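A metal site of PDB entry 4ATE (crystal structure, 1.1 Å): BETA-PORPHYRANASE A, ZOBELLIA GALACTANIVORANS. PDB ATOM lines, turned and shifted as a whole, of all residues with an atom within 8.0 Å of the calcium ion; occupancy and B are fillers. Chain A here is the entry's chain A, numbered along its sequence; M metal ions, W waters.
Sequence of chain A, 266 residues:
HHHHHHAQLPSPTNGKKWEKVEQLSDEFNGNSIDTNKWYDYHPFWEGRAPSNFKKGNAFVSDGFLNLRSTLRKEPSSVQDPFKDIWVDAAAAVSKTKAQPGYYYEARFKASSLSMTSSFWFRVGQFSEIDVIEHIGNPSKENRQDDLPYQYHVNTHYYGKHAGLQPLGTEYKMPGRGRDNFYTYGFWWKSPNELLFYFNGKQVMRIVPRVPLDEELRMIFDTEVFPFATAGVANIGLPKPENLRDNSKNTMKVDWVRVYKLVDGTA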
ATOM      1  N   ASP A  26     -13.302  19.588  26.013  1.00  0.00           N
ATOM      2  CA  ASP A  26     -14.463  19.108  26.814  1.00  0.00           C
ATOM      3  C   ASP A  26     -15.416  18.463  25.883  1.00  0.00           C
ATOM      4  O   ASP A  26     -15.824  19.047  24.842  1.00  0.00           O
ATOM      5  CB  ASP A  26     -15.080  20.289  27.590  1.00  0.00           C
ATOM      6  CG  ASP A  26     -15.821  19.872  28.800  1.00  0.00           C
ATOM      7  OD1 ASP A  26     -16.433  18.801  28.805  1.00  0.00           O
ATOM      8  OD2 ASP A  26     -15.896  20.691  29.762  1.00  0.00           O
ATOM      9  N   GLU A  27     -15.817  17.238  26.223  1.00  0.00           N
ATOM     10  CA  GLU A  27     -16.877  16.527  25.488  1.00  0.00           C
ATOM     11  C   GLU A  27     -18.225  16.967  25.957  1.00  0.00           C
ATOM     12  O   GLU A  27     -19.234  16.557  25.358  1.00  0.00           O
ATOM     13  CB  GLU A  27     -16.712  14.995  25.619  1.00  0.00           C
ATOM     14  CG  GLU A  27     -15.384  14.547  25.081  1.00  0.00           C
ATOM     15  CD  GLU A  27     -15.267  14.753  23.581  1.00  0.00           C
ATOM     16  OE1 GLU A  27     -16.239  14.402  22.821  1.00  0.00           O
ATOM     17  OE2 GLU A  27     -14.237  15.274  23.110  1.00  0.00           O
ATOM     18  N   PHE A  28     -18.336  17.727  27.015  1.00  0.00           N
ATOM     19  CA  PHE A  28     -19.598  18.267  27.517  1.00  0.00           C
ATOM     20  C   PHE A  28     -20.627  17.186  27.770  1.00  0.00           C
ATOM     21  O   PHE A  28     -21.828  17.332  27.554  1.00  0.00           O
ATOM     22  CB  PHE A  28     -20.166  19.336  26.560  1.00  0.00           C
ATOM     23  CG  PHE A  28     -19.278  20.543  26.422  1.00  0.00           C
ATOM     24  CD1 PHE A  28     -18.840  21.257  27.563  1.00  0.00           C
ATOM     25  CD2 PHE A  28     -18.901  20.930  25.129  1.00  0.00           C
ATOM     26  CE1 PHE A  28     -18.043  22.395  27.371  1.00  0.00           C
ATOM     27  CE2 PHE A  28     -18.082  22.033  24.943  1.00  0.00           C
ATOM     28  CZ  PHE A  28     -17.660  22.763  26.064  1.00  0.00           C
ATOM     29  N   ASN A  29     -20.149  16.050  28.296  1.00  0.00           N
ATOM     30  CA  ASN A  29     -21.012  14.885  28.481  1.00  0.00           C
ATOM     31  C   ASN A  29     -21.352  14.728  29.941  1.00  0.00           C
ATOM     32  O   ASN A  29     -22.012  13.722  30.282  1.00  0.00           O
ATOM     33  CB  ASN A  29     -20.368  13.606  27.890  1.00  0.00           C
ATOM     34  CG  ASN A  29     -20.326  13.631  26.352  1.00  0.00           C
ATOM     35  OD1 ASN A  29     -21.052  14.287  25.741  1.00  0.00           O
ATOM     36  ND2 ASN A  29     -19.354  12.831  25.869  1.00  0.00           N
ATOM     37  N   GLY A  30     -20.992  15.628  30.821  1.00  0.00           N
ATOM     38  CA  GLY A  30     -21.307  15.514  32.249  1.00  0.00           C
ATOM     39  C   GLY A  30     -22.649  16.076  32.579  1.00  0.00           C
ATOM     40  O   GLY A  30     -23.460  16.450  31.720  1.00  0.00           O
ATOM     41  N   VAL A  60     -24.387  22.710  30.732  1.00  0.00           N
ATOM     42  CA  VAL A  60     -24.104  21.435  30.150  1.00  0.00           C
ATOM     43  C   VAL A  60     -25.147  20.423  30.466  1.00  0.00           C
ATOM     44  O   VAL A  60     -25.478  20.217  31.657  1.00  0.00           O
ATOM     45  CB  VAL A  60     -22.669  20.972  30.576  1.00  0.00           C
ATOM     46  CG1 VAL A  60     -22.407  19.493  30.186  1.00  0.00           C
ATOM     47  CG2 VAL A  60     -21.596  21.879  29.962  1.00  0.00           C
ATOM     48  N   SER A  61     -25.672  19.748  29.465  1.00  0.00           N
ATOM     49  CA  SER A  61     -26.595  18.656  29.653  1.00  0.00           C
ATOM     50  C   SER A  61     -26.877  18.017  28.304  1.00  0.00           C
ATOM     51  O   SER A  61     -26.703  18.590  27.215  1.00  0.00           O
ATOM     52  CB  SER A  61     -27.859  19.129  30.341  1.00  0.00           C
ATOM     53  OG  SER A  61     -28.566  19.989  29.523  1.00  0.00           O
ATOM     54  N   ASP A  62     -27.271  16.753  28.403  1.00  0.00           N
ATOM     55  CA  ASP A  62     -27.643  15.969  27.251  1.00  0.00           C
ATOM     56  C   ASP A  62     -26.549  15.805  26.191  1.00  0.00           C
ATOM     57  O   ASP A  62     -26.826  15.535  25.030  1.00  0.00           O
ATOM     58  CB  ASP A  62     -28.983  16.438  26.717  1.00  0.00           C
ATOM     59  CG  ASP A  62     -30.094  16.162  27.713  1.00  0.00           C
ATOM     60  OD1 ASP A  62     -30.125  15.024  28.210  1.00  0.00           O
ATOM     61  OD2 ASP A  62     -30.850  17.072  28.047  1.00  0.00           O
ATOM     62  N   GLY A  63     -25.293  15.896  26.644  1.00  0.00           N
ATOM     63  CA  GLY A  63     -24.121  15.710  25.742  1.00  0.00           C
ATOM     64  C   GLY A  63     -23.567  17.020  25.118  1.00  0.00           C
ATOM     65  O   GLY A  63     -22.636  16.984  24.352  1.00  0.00           O
ATOM     66  N   PHE A  64     -24.209  18.139  25.450  1.00  0.00           N
ATOM     67  CA  PHE A  64     -23.873  19.468  24.872  1.00  0.00           C
ATOM     68  C   PHE A  64     -23.525  20.492  25.913  1.00  0.00           C
ATOM     69  O   PHE A  64     -24.095  20.491  27.011  1.00  0.00           O
ATOM     70  CB  PHE A  64     -25.016  20.031  24.000  1.00  0.00           C
ATOM     71  CG  PHE A  64     -25.541  19.096  23.006  1.00  0.00           C
ATOM     72  CD1 PHE A  64     -24.815  18.805  21.818  1.00  0.00           C
ATOM     73  CD2 PHE A  64     -26.769  18.420  23.236  1.00  0.00           C
ATOM     74  CE1 PHE A  64     -25.242  17.900  20.859  1.00  0.00           C
ATOM     75  CE2 PHE A  64     -27.205  17.511  22.242  1.00  0.00           C
ATOM     76  CZ  PHE A  64     -26.469  17.202  21.082  1.00  0.00           C
ATOM     77  N   LEU A  65     -22.687  21.453  25.487  1.00  0.00           N
ATOM     78  CA  LEU A  65     -22.753  22.785  26.085  1.00  0.00           C
ATOM     79  C   LEU A  65     -23.880  23.526  25.348  1.00  0.00           C
ATOM     80  O   LEU A  65     -23.798  23.771  24.120  1.00  0.00           O
ATOM     81  CB  LEU A  65     -21.417  23.537  25.951  1.00  0.00           C
ATOM     82  CG  LEU A  65     -21.455  24.989  26.401  1.00  0.00           C
ATOM     83  CD1 LEU A  65     -21.688  25.125  27.921  1.00  0.00           C
ATOM     84  CD2 LEU A  65     -20.114  25.659  25.971  1.00  0.00           C
ATOM     85  N   ARG A 107     -17.484  21.373  17.473  1.00  0.00           N
ATOM     86  CA  ARG A 107     -18.585  20.818  16.665  1.00  0.00           C
ATOM     87  C   ARG A 107     -19.862  21.362  17.274  1.00  0.00           C
ATOM     88  O   ARG A 107     -20.183  21.052  18.439  1.00  0.00           O
ATOM     89  CB  ARG A 107     -18.537  19.303  16.607  1.00  0.00           C
ATOM     90  CG  ARG A 107     -19.755  18.700  15.889  1.00  0.00           C
ATOM     91  CD  ARG A 107     -19.326  17.267  15.434  1.00  0.00           C
ATOM     92  NE  ARG A 107     -20.338  16.652  14.572  1.00  0.00           N
ATOM     93  CZ  ARG A 107     -20.376  16.815  13.278  1.00  0.00           C
ATOM     94  NH1 ARG A 107     -19.432  17.551  12.588  1.00  0.00           N
ATOM     95  NH2 ARG A 107     -21.368  16.163  12.628  1.00  0.00           N
ATOM     96  N   VAL A 253     -23.178  22.913  21.481  1.00  0.00           N
ATOM     97  CA  VAL A 253     -21.785  22.523  21.220  1.00  0.00           C
ATOM     98  C   VAL A 253     -21.608  21.070  21.660  1.00  0.00           C
ATOM     99  O   VAL A 253     -21.675  20.799  22.916  1.00  0.00           O
ATOM    100  CB  VAL A 253     -20.765  23.424  21.868  1.00  0.00           C
ATOM    101  CG1 VAL A 253     -19.372  23.023  21.486  1.00  0.00           C
ATOM    102  CG2 VAL A 253     -21.051  24.929  21.556  1.00  0.00           C
ATOM    103  N   ASP A 254     -21.440  20.138  20.786  1.00  0.00           N
ATOM    104  CA  ASP A 254     -21.233  18.708  21.152  1.00  0.00           C
ATOM    105  C   ASP A 254     -19.886  18.586  21.881  1.00  0.00           C
ATOM    106  O   ASP A 254     -19.775  17.816  22.867  1.00  0.00           O
ATOM    107  CB  ASP A 254     -21.337  17.871  19.929  1.00  0.00           C
ATOM    108  CG  ASP A 254     -21.362  16.358  20.246  1.00  0.00           C
ATOM    109  OD1 ASP A 254     -21.436  15.987  21.399  1.00  0.00           O
ATOM    110  OD2 ASP A 254     -21.328  15.630  19.243  1.00  0.00           O
ATOM    111  N   TRP A 255     -18.853  19.270  21.412  1.00  0.00           N
ATOM    112  CA  TRP A 255     -17.525  19.131  22.029  1.00  0.00           C
ATOM    113  C   TRP A 255     -16.658  20.266  21.511  1.00  0.00           C
ATOM    114  O   TRP A 255     -16.901  20.852  20.442  1.00  0.00           O
ATOM    115  CB  TRP A 255     -16.896  17.747  21.705  1.00  0.00           C
ATOM    116  CG  TRP A 255     -16.950  17.267  20.297  1.00  0.00           C
ATOM    117  CD1 TRP A 255     -17.786  16.235  19.879  1.00  0.00           C
ATOM    118  CD2 TRP A 255     -16.114  17.604  19.173  1.00  0.00           C
ATOM    119  NE1 TRP A 255     -17.530  15.978  18.573  1.00  0.00           N
ATOM    120  CE2 TRP A 255     -16.499  16.781  18.116  1.00  0.00           C
ATOM    121  CE3 TRP A 255     -15.123  18.561  18.956  1.00  0.00           C
ATOM    122  CZ2 TRP A 255     -15.893  16.786  16.865  1.00  0.00           C
ATOM    123  CZ3 TRP A 255     -14.512  18.634  17.717  1.00  0.00           C
ATOM    124  CH2 TRP A 255     -14.885  17.762  16.666  1.00  0.00           C
ATOM    125  N   VAL A 256     -15.603  20.511  22.289  1.00  0.00           N
ATOM    126  CA  VAL A 256     -14.479  21.351  21.836  1.00  0.00           C
ATOM    127  C   VAL A 256     -13.211  20.551  22.116  1.00  0.00           C
ATOM    128  O   VAL A 256     -13.094  19.923  23.218  1.00  0.00           O
ATOM    129  CB  VAL A 256     -14.469  22.735  22.497  1.00  0.00           C
ATOM    130  CG1 VAL A 256     -14.345  22.703  24.056  1.00  0.00           C
ATOM    131  CG2 VAL A 256     -13.431  23.660  21.914  1.00  0.00           C
ATOM    132  N   ARG A 257     -12.290  20.543  21.208  1.00  0.00           N
ATOM    133  CA  ARG A 257     -11.035  19.781  21.360  1.00  0.00           C
ATOM    134  C   ARG A 257      -9.912  20.675  20.884  1.00  0.00           C
ATOM    135  O   ARG A 257     -10.003  21.324  19.836  1.00  0.00           O
ATOM    136  CB  ARG A 257     -11.069  18.507  20.520  1.00  0.00           C
ATOM    137  CG  ARG A 257     -12.175  17.512  20.976  1.00  0.00           C
ATOM    138  CD  ARG A 257     -12.374  16.430  19.953  1.00  0.00           C
ATOM    139  NE  ARG A 257     -13.472  15.524  20.391  1.00  0.00           N
ATOM    140  CZ  ARG A 257     -14.153  14.677  19.593  1.00  0.00           C
ATOM    141  NH1 ARG A 257     -13.758  14.531  18.364  1.00  0.00           N
ATOM    142  NH2 ARG A 257     -15.153  13.995  20.087  1.00  0.00           N
HETATM  143 CA    CA M   1     -20.780  15.802  23.699  1.00  0.00          CA
HETATM  144  O   HOH W   1     -22.143  13.852  23.232  1.00  0.00           O
HETATM  145  O   HOH W   2     -19.002  14.437  22.888  1.00  0.00           O
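The backbone NH (N) of Asp 254 is in hydrogen-bond range of the backbone carbonyl oxygen (O) of Arg 107 (2.8 Å). The side-chain carboxylate (OE2) of Glu 27 is in salt-bridge range of the guanidinium group (NE) of Arg 257, at 2.8 Å.
Of the 17 residues printed, 4 come within 4 Å of the calcium ion.
The calcium ion is bound by O of Gly 63 (2.3 Å), water W2 (2.4 Å), O of Glu 27 (2.4 Å), OD1 of Asp 254 (2.4 Å), O of Asp 254 (2.4 Å), water W1 (2.4 Å) and OD1 of Asn 29 (2.6 Å).
Water W2 bridges the side-chain carboxylate of Glu 27 (2.8 Å) and the side-chain amide nitrogen of Asn 29 (3.4 Å).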
